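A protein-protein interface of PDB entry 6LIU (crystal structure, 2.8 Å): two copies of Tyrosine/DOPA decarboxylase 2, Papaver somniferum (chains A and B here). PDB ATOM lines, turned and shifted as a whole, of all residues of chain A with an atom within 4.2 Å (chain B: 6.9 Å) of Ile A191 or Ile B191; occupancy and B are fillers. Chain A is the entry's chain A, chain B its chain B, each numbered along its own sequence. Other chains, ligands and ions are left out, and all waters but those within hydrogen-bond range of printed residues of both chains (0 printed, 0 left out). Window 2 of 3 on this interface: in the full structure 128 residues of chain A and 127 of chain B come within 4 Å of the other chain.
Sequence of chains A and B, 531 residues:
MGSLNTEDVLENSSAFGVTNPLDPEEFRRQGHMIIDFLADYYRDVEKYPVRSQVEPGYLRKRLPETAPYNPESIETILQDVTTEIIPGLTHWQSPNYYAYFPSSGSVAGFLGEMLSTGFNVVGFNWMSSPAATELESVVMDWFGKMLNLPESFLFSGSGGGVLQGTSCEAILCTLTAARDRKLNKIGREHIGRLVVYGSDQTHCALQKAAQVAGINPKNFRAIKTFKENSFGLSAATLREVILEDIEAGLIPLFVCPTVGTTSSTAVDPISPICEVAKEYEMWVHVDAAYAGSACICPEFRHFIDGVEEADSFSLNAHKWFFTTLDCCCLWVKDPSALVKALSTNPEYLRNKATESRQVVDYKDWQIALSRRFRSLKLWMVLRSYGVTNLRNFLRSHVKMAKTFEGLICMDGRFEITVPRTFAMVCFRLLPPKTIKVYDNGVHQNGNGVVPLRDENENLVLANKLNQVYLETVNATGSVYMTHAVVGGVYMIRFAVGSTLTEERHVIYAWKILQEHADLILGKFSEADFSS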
ATOM      1  N   LEU A 183     -22.080 -29.078  30.294  1.00  0.00           N
ATOM      2  CA  LEU A 183     -22.578 -28.274  29.184  1.00  0.00           C
ATOM      3  C   LEU A 183     -24.069 -28.470  28.941  1.00  0.00           C
ATOM      4  O   LEU A 183     -24.703 -27.589  28.352  1.00  0.00           O
ATOM      5  CB  LEU A 183     -21.794 -28.585  27.908  1.00  0.00           C
ATOM      6  CG  LEU A 183     -20.367 -28.031  27.847  1.00  0.00           C
ATOM      7  CD1 LEU A 183     -19.764 -28.248  26.475  1.00  0.00           C
ATOM      8  CD2 LEU A 183     -20.326 -26.557  28.222  1.00  0.00           C
ATOM      9  N   ARG A 188     -24.269 -25.406  25.729  1.00  0.00           N
ATOM     10  CA  ARG A 188     -23.134 -25.909  24.957  1.00  0.00           C
ATOM     11  C   ARG A 188     -22.124 -24.814  24.634  1.00  0.00           C
ATOM     12  O   ARG A 188     -20.934 -25.099  24.457  1.00  0.00           O
ATOM     13  CB  ARG A 188     -23.626 -26.561  23.661  1.00  0.00           C
ATOM     14  CG  ARG A 188     -24.314 -27.899  23.860  1.00  0.00           C
ATOM     15  CD  ARG A 188     -23.295 -28.991  24.098  1.00  0.00           C
ATOM     16  NE  ARG A 188     -23.911 -30.312  24.182  1.00  0.00           N
ATOM     17  CZ  ARG A 188     -23.236 -31.430  24.427  1.00  0.00           C
ATOM     18  NH1 ARG A 188     -21.921 -31.382  24.610  1.00  0.00           N
ATOM     19  NH2 ARG A 188     -23.872 -32.592  24.490  1.00  0.00           N
ATOM     20  N   GLU A 189     -22.572 -23.559  24.558  1.00  0.00           N
ATOM     21  CA  GLU A 189     -21.714 -22.460  24.134  1.00  0.00           C
ATOM     22  C   GLU A 189     -20.560 -22.192  25.093  1.00  0.00           C
ATOM     23  O   GLU A 189     -19.655 -21.425  24.742  1.00  0.00           O
ATOM     24  CB  GLU A 189     -22.550 -21.190  23.972  1.00  0.00           C
ATOM     25  CG  GLU A 189     -23.144 -20.664  25.272  1.00  0.00           C
ATOM     26  CD  GLU A 189     -24.504 -21.266  25.592  1.00  0.00           C
ATOM     27  OE1 GLU A 189     -24.849 -22.323  25.016  1.00  0.00           O
ATOM     28  OE2 GLU A 189     -25.227 -20.678  26.428  1.00  0.00           O
ATOM     29  N   HIS A 190     -20.560 -22.797  26.281  1.00  0.00           N
ATOM     30  CA  HIS A 190     -19.543 -22.531  27.289  1.00  0.00           C
ATOM     31  C   HIS A 190     -18.415 -23.555  27.276  1.00  0.00           C
ATOM     32  O   HIS A 190     -17.643 -23.625  28.239  1.00  0.00           O
ATOM     33  CB  HIS A 190     -20.186 -22.462  28.675  1.00  0.00           C
ATOM     34  CG  HIS A 190     -21.137 -21.318  28.835  1.00  0.00           C
ATOM     35  ND1 HIS A 190     -22.463 -21.491  29.170  1.00  0.00           N
ATOM     36  CD2 HIS A 190     -20.955 -19.983  28.693  1.00  0.00           C
ATOM     37  CE1 HIS A 190     -23.056 -20.313  29.230  1.00  0.00           C
ATOM     38  NE2 HIS A 190     -22.163 -19.381  28.944  1.00  0.00           N
ATOM     39  N   ILE A 191     -18.300 -24.346  26.203  1.00  0.00           N
ATOM     40  CA  ILE A 191     -17.221 -25.328  26.120  1.00  0.00           C
ATOM     41  C   ILE A 191     -15.862 -24.644  26.194  1.00  0.00           C
ATOM     42  O   ILE A 191     -14.900 -25.213  26.727  1.00  0.00           O
ATOM     43  CB  ILE A 191     -17.358 -26.180  24.839  1.00  0.00           C
ATOM     44  CG1 ILE A 191     -16.299 -27.288  24.812  1.00  0.00           C
ATOM     45  CG2 ILE A 191     -17.268 -25.315  23.587  1.00  0.00           C
ATOM     46  CD1 ILE A 191     -16.366 -28.172  23.581  1.00  0.00           C
ATOM     47  N   GLY A 192     -15.761 -23.411  25.692  1.00  0.00           N
ATOM     48  CA  GLY A 192     -14.511 -22.677  25.677  1.00  0.00           C
ATOM     49  C   GLY A 192     -14.051 -22.168  27.018  1.00  0.00           C
ATOM     50  O   GLY A 192     -12.991 -21.540  27.093  1.00  0.00           O
ATOM     51  N   ARG A 193     -14.817 -22.425  28.079  1.00  0.00           N
ATOM     52  CA  ARG A 193     -14.471 -22.000  29.426  1.00  0.00           C
ATOM     53  C   ARG A 193     -14.138 -23.159  30.355  1.00  0.00           C
ATOM     54  O   ARG A 193     -13.643 -22.919  31.463  1.00  0.00           O
ATOM     55  CB  ARG A 193     -15.621 -21.179  30.036  1.00  0.00           C
ATOM     56  CG  ARG A 193     -16.006 -19.948  29.222  1.00  0.00           C
ATOM     57  CD  ARG A 193     -16.753 -18.906  30.066  1.00  0.00           C
ATOM     58  NE  ARG A 193     -18.100 -19.338  30.422  1.00  0.00           N
ATOM     59  CZ  ARG A 193     -18.562 -19.395  31.668  1.00  0.00           C
ATOM     60  NH1 ARG A 193     -17.779 -19.043  32.683  1.00  0.00           N
ATOM     61  NH2 ARG A 193     -19.806 -19.805  31.898  1.00  0.00           N
ATOM     62  N   LEU A 194     -14.397 -24.397  29.938  1.00  0.00           N
ATOM     63  CA  LEU A 194     -14.168 -25.548  30.800  1.00  0.00           C
ATOM     64  C   LEU A 194     -12.677 -25.765  31.024  1.00  0.00           C
ATOM     65  O   LEU A 194     -11.870 -25.667  30.095  1.00  0.00           O
ATOM     66  CB  LEU A 194     -14.795 -26.797  30.188  1.00  0.00           C
ATOM     67  CG  LEU A 194     -16.283 -26.667  29.875  1.00  0.00           C
ATOM     68  CD1 LEU A 194     -16.832 -27.979  29.338  1.00  0.00           C
ATOM     69  CD2 LEU A 194     -17.030 -26.228  31.124  1.00  0.00           C
ATOM     70  N   ALA A 213     -11.507 -33.853  23.201  1.00  0.00           N
ATOM     71  CA  ALA A 213     -12.831 -33.523  23.720  1.00  0.00           C
ATOM     72  C   ALA A 213     -13.251 -32.081  23.454  1.00  0.00           C
ATOM     73  O   ALA A 213     -14.377 -31.715  23.812  1.00  0.00           O
ATOM     74  CB  ALA A 213     -12.887 -33.801  25.223  1.00  0.00           C
ATOM     75  N   GLY A 214     -12.398 -31.258  22.851  1.00  0.00           N
ATOM     76  CA  GLY A 214     -12.748 -29.880  22.581  1.00  0.00           C
ATOM     77  C   GLY A 214     -12.423 -28.900  23.686  1.00  0.00           C
ATOM     78  O   GLY A 214     -12.926 -27.770  23.656  1.00  0.00           O
ATOM     79  N   ARG B 179     -10.846 -30.349  12.278  1.00  0.00           N
ATOM     80  CA  ARG B 179     -11.288 -29.285  13.174  1.00  0.00           C
ATOM     81  C   ARG B 179     -10.125 -28.383  13.582  1.00  0.00           C
ATOM     82  O   ARG B 179     -10.247 -27.153  13.573  1.00  0.00           O
ATOM     83  CB  ARG B 179     -11.965 -29.906  14.397  1.00  0.00           C
ATOM     84  CG  ARG B 179     -12.413 -28.934  15.458  1.00  0.00           C
ATOM     85  CD  ARG B 179     -12.508 -29.634  16.802  1.00  0.00           C
ATOM     86  NE  ARG B 179     -11.185 -29.989  17.304  1.00  0.00           N
ATOM     87  CZ  ARG B 179     -10.966 -30.768  18.359  1.00  0.00           C
ATOM     88  NH1 ARG B 179     -11.986 -31.282  19.034  1.00  0.00           N
ATOM     89  NH2 ARG B 179      -9.722 -31.033  18.739  1.00  0.00           N
ATOM     90  N   LEU B 183      -9.771 -24.380  12.893  1.00  0.00           N
ATOM     91  CA  LEU B 183      -9.814 -23.496  14.052  1.00  0.00           C
ATOM     92  C   LEU B 183      -8.484 -22.783  14.274  1.00  0.00           C
ATOM     93  O   LEU B 183      -8.466 -21.672  14.813  1.00  0.00           O
ATOM     94  CB  LEU B 183     -10.211 -24.284  15.301  1.00  0.00           C
ATOM     95  CG  LEU B 183     -11.671 -24.729  15.411  1.00  0.00           C
ATOM     96  CD1 LEU B 183     -11.953 -25.211  16.820  1.00  0.00           C
ATOM     97  CD2 LEU B 183     -12.635 -23.611  15.016  1.00  0.00           C
ATOM     98  N   ILE B 186      -8.910 -19.678  12.054  1.00  0.00           N
ATOM     99  CA  ILE B 186      -9.972 -18.731  12.366  1.00  0.00           C
ATOM    100  C   ILE B 186     -10.162 -18.513  13.859  1.00  0.00           C
ATOM    101  O   ILE B 186     -10.944 -17.626  14.240  1.00  0.00           O
ATOM    102  CB  ILE B 186     -11.305 -19.165  11.725  1.00  0.00           C
ATOM    103  CG1 ILE B 186     -11.895 -20.346  12.493  1.00  0.00           C
ATOM    104  CG2 ILE B 186     -11.094 -19.544  10.276  1.00  0.00           C
ATOM    105  CD1 ILE B 186     -13.259 -20.748  12.015  1.00  0.00           C
ATOM    106  N   GLY B 187      -9.499 -19.280  14.707  1.00  0.00           N
ATOM    107  CA  GLY B 187      -9.623 -19.097  16.145  1.00  0.00           C
ATOM    108  C   GLY B 187     -10.479 -20.179  16.779  1.00  0.00           C
ATOM    109  O   GLY B 187     -11.516 -20.579  16.236  1.00  0.00           O
ATOM    110  N   ARG B 188     -10.048 -20.651  17.954  1.00  0.00           N
ATOM    111  CA  ARG B 188     -10.766 -21.712  18.654  1.00  0.00           C
ATOM    112  C   ARG B 188     -12.190 -21.315  19.021  1.00  0.00           C
ATOM    113  O   ARG B 188     -13.013 -22.192  19.308  1.00  0.00           O
ATOM    114  CB  ARG B 188     -10.001 -22.112  19.917  1.00  0.00           C
ATOM    115  CG  ARG B 188      -8.625 -22.704  19.649  1.00  0.00           C
ATOM    116  CD  ARG B 188      -8.702 -23.803  18.606  1.00  0.00           C
ATOM    117  NE  ARG B 188      -7.384 -24.278  18.195  1.00  0.00           N
ATOM    118  CZ  ARG B 188      -6.956 -25.526  18.364  1.00  0.00           C
ATOM    119  NH1 ARG B 188      -7.745 -26.424  18.940  1.00  0.00           N
ATOM    120  NH2 ARG B 188      -5.742 -25.876  17.956  1.00  0.00           N
ATOM    121  N   GLU B 189     -12.501 -20.018  19.012  1.00  0.00           N
ATOM    122  CA  GLU B 189     -13.798 -19.525  19.457  1.00  0.00           C
ATOM    123  C   GLU B 189     -14.946 -19.933  18.541  1.00  0.00           C
ATOM    124  O   GLU B 189     -16.107 -19.786  18.937  1.00  0.00           O
ATOM    125  CB  GLU B 189     -13.754 -17.998  19.582  1.00  0.00           C
ATOM    126  CG  GLU B 189     -13.042 -17.288  18.427  1.00  0.00           C
ATOM    127  CD  GLU B 189     -11.545 -17.137  18.644  1.00  0.00           C
ATOM    128  OE1 GLU B 189     -11.014 -17.716  19.616  1.00  0.00           O
ATOM    129  OE2 GLU B 189     -10.895 -16.441  17.835  1.00  0.00           O
ATOM    130  N   HIS B 190     -14.663 -20.439  17.341  1.00  0.00           N
ATOM    131  CA  HIS B 190     -15.700 -20.764  16.371  1.00  0.00           C
ATOM    132  C   HIS B 190     -16.040 -22.253  16.334  1.00  0.00           C
ATOM    133  O   HIS B 190     -16.654 -22.710  15.365  1.00  0.00           O
ATOM    134  CB  HIS B 190     -15.283 -20.296  14.976  1.00  0.00           C
ATOM    135  CG  HIS B 190     -15.020 -18.826  14.882  1.00  0.00           C
ATOM    136  ND1 HIS B 190     -15.938 -17.878  15.279  1.00  0.00           N
ATOM    137  CD2 HIS B 190     -13.942 -18.141  14.430  1.00  0.00           C
ATOM    138  CE1 HIS B 190     -15.436 -16.672  15.080  1.00  0.00           C
ATOM    139  NE2 HIS B 190     -14.226 -16.804  14.566  1.00  0.00           N
ATOM    140  N   ILE B 191     -15.661 -23.018  17.363  1.00  0.00           N
ATOM    141  CA  ILE B 191     -15.926 -24.456  17.337  1.00  0.00           C
ATOM    142  C   ILE B 191     -17.421 -24.718  17.213  1.00  0.00           C
ATOM    143  O   ILE B 191     -17.848 -25.627  16.491  1.00  0.00           O
ATOM    144  CB  ILE B 191     -15.320 -25.146  18.576  1.00  0.00           C
ATOM    145  CG1 ILE B 191     -15.430 -26.668  18.442  1.00  0.00           C
ATOM    146  CG2 ILE B 191     -15.986 -24.673  19.864  1.00  0.00           C
ATOM    147  CD1 ILE B 191     -14.852 -27.430  19.627  1.00  0.00           C
ATOM    148  N   GLY B 192     -18.240 -23.896  17.874  1.00  0.00           N
ATOM    149  CA  GLY B 192     -19.685 -24.010  17.849  1.00  0.00           C
ATOM    150  C   GLY B 192     -20.343 -23.680  16.526  1.00  0.00           C
ATOM    151  O   GLY B 192     -21.571 -23.778  16.426  1.00  0.00           O
ATOM    152  N   ARG B 193     -19.571 -23.292  15.510  1.00  0.00           N
ATOM    153  CA  ARG B 193     -20.114 -23.061  14.181  1.00  0.00           C
ATOM    154  C   ARG B 193     -19.774 -24.165  13.188  1.00  0.00           C
ATOM    155  O   ARG B 193     -20.336 -24.174  12.087  1.00  0.00           O
ATOM    156  CB  ARG B 193     -19.623 -21.711  13.629  1.00  0.00           C
ATOM    157  CG  ARG B 193     -20.254 -20.496  14.307  1.00  0.00           C
ATOM    158  CD  ARG B 193     -19.395 -19.241  14.137  1.00  0.00           C
ATOM    159  NE  ARG B 193     -19.628 -18.582  12.853  1.00  0.00           N
ATOM    160  CZ  ARG B 193     -18.772 -17.743  12.276  1.00  0.00           C
ATOM    161  NH1 ARG B 193     -17.620 -17.454  12.869  1.00  0.00           N
ATOM    162  NH2 ARG B 193     -19.067 -17.192  11.106  1.00  0.00           N
ATOM    163  N   LEU B 194     -18.891 -25.097  13.546  1.00  0.00           N
ATOM    164  CA  LEU B 194     -18.457 -26.125  12.609  1.00  0.00           C
ATOM    165  C   LEU B 194     -19.561 -27.148  12.362  1.00  0.00           C
ATOM    166  O   LEU B 194     -20.229 -27.607  13.292  1.00  0.00           O
ATOM    167  CB  LEU B 194     -17.204 -26.820  13.137  1.00  0.00           C
ATOM    168  CG  LEU B 194     -16.038 -25.893  13.484  1.00  0.00           C
ATOM    169  CD1 LEU B 194     -14.834 -26.701  13.955  1.00  0.00           C
ATOM    170  CD2 LEU B 194     -15.674 -25.020  12.288  1.00  0.00           C
ATOM    171  N   VAL B 195     -19.740 -27.517  11.097  1.00  0.00           N
ATOM    172  CA  VAL B 195     -20.839 -28.373  10.667  1.00  0.00           C
ATOM    173  C   VAL B 195     -20.260 -29.612   9.998  1.00  0.00           C
ATOM    174  O   VAL B 195     -19.491 -29.501   9.035  1.00  0.00           O
ATOM    175  CB  VAL B 195     -21.786 -27.632   9.711  1.00  0.00           C
ATOM    176  CG1 VAL B 195     -22.907 -28.554   9.261  1.00  0.00           C
ATOM    177  CG2 VAL B 195     -22.342 -26.393  10.393  1.00  0.00           C
ATOM    178  N   ALA B 213     -15.666 -35.021  19.525  1.00  0.00           N
ATOM    179  CA  ALA B 213     -14.768 -33.964  19.077  1.00  0.00           C
ATOM    180  C   ALA B 213     -15.265 -32.560  19.409  1.00  0.00           C
ATOM    181  O   ALA B 213     -14.625 -31.582  19.006  1.00  0.00           O
ATOM    182  CB  ALA B 213     -14.533 -34.083  17.570  1.00  0.00           C
ATOM    183  N   GLY B 214     -16.375 -32.426  20.129  1.00  0.00           N
ATOM    184  CA  GLY B 214     -16.852 -31.126  20.544  1.00  0.00           C
ATOM    185  C   GLY B 214     -17.729 -30.407  19.544  1.00  0.00           C
ATOM    186  O   GLY B 214     -18.097 -29.250  19.792  1.00  0.00           O
ATOM    187  N   ILE B 215     -18.055 -31.039  18.414  1.00  0.00           N
ATOM    188  CA  ILE B 215     -19.003 -30.450  17.478  1.00  0.00           C
ATOM    189  C   ILE B 215     -20.356 -30.320  18.161  1.00  0.00           C
ATOM    190  O   ILE B 215     -20.777 -31.204  18.918  1.00  0.00           O
ATOM    191  CB  ILE B 215     -19.096 -31.302  16.203  1.00  0.00           C
ATOM    192  CG1 ILE B 215     -17.743 -31.340  15.492  1.00  0.00           C
ATOM    193  CG2 ILE B 215     -20.183 -30.787  15.268  1.00  0.00           C
ATOM    194  CD1 ILE B 215     -17.238 -29.976  15.069  1.00  0.00           C
ATOM    195  N   ASN B 216     -21.031 -29.199  17.925  1.00  0.00           N
ATOM    196  CA  ASN B 216     -22.338 -28.989  18.533  1.00  0.00           C
ATOM    197  C   ASN B 216     -23.325 -30.014  17.987  1.00  0.00           C
ATOM    198  O   ASN B 216     -23.393 -30.209  16.768  1.00  0.00           O
ATOM    199  CB  ASN B 216     -22.846 -27.573  18.266  1.00  0.00           C
ATOM    200  CG  ASN B 216     -24.072 -27.234  19.093  1.00  0.00           C
ATOM    201  OD1 ASN B 216     -25.182 -27.664  18.782  1.00  0.00           O
ATOM    202  ND2 ASN B 216     -23.874 -26.471  20.164  1.00  0.00           N
ATOM    203  N   ASN B 219     -25.272 -29.193  14.915  1.00  0.00           N
ATOM    204  CA  ASN B 219     -24.521 -28.933  13.693  1.00  0.00           C
ATOM    205  C   ASN B 219     -24.092 -30.227  13.009  1.00  0.00           C
ATOM    206  O   ASN B 219     -23.144 -30.228  12.214  1.00  0.00           O
ATOM    207  CB  ASN B 219     -23.312 -28.045  13.991  1.00  0.00           C
ATOM    208  CG  ASN B 219     -23.700 -26.592  14.187  1.00  0.00           C
ATOM    209  OD1 ASN B 219     -24.731 -26.143  13.682  1.00  0.00           O
ATOM    210  ND2 ASN B 219     -22.878 -25.849  14.926  1.00  0.00           N
ATOM    211  N   ILE B 251     -20.181 -22.700   9.762  1.00  0.00           N
ATOM    212  CA  ILE B 251     -18.953 -22.950   9.013  1.00  0.00           C
ATOM    213  C   ILE B 251     -18.905 -24.412   8.584  1.00  0.00           C
ATOM    214  O   ILE B 251     -18.724 -25.296   9.431  1.00  0.00           O
ATOM    215  CB  ILE B 251     -17.714 -22.592   9.846  1.00  0.00           C
ATOM    216  CG1 ILE B 251     -17.763 -21.123  10.269  1.00  0.00           C
ATOM    217  CG2 ILE B 251     -16.438 -22.896   9.071  1.00  0.00           C
ATOM    218  CD1 ILE B 251     -16.775 -20.772  11.349  1.00  0.00           C
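The backbone carbonyl oxygen (O) of Leu A183 lies within hydrogen-bond range of the backbone NH (N) of Arg A188 (3.4 Å).
O of Ala B213 is in hydrogen-bond range of NH1 of Arg B179 (2.7 Å).
Printed residues of chain B within 4 Å of Arg A188: Asn B216 (3.5 Å).
Printed residues of chain B within 4 Å of Ile A191: Ile B191 (3.99 Å).
Of the printed residues of chain B, Gly A214 touches Arg B179 (3.8 Å).
Printed residues of chain A within 4 Å of Arg B179: Gly A214 (3.8 Å).
Of the printed residues of chain A, Ile B191 touches Ile A191.
Ile B215 touches none of the printed residues of chain A.
Printed residues of chain A within 4 Å of Asn B216: Arg A188 (3.5 Å).
The nearest printed residue of chain B that does not touch Ile A191 is Gly B214 (4.3 Å).
The nearest printed residue of chain A that does not touch Ile B191 is Gly A214 (4.4 Å).
Among the printed residues, merely in contact across the chains: Arg A188 with Asn B216 (3.5 Å), Gly A214 with Arg B179 (3.8 Å) and Ile A191 with Ile B191 (3.99 Å).
Ile A191 touches its own counterpart, Ile B191.
Printed residues of chain A that touch a printed residue of chain B: Arg A188, Ile A191 and Gly A214.
Of the 18 printed residues of chain B, 3 touch a printed residue of chain A.
Hydrophobic or aromatic side chains of chain B that line the printed part of chain A: Ile B191.
Among the printed residues, 3 pairs touch across the chains.
Among the printed residues, no Asp or Glu carboxylate lies within 4 Å of a Lys or Arg side-chain nitrogen of the other chain.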
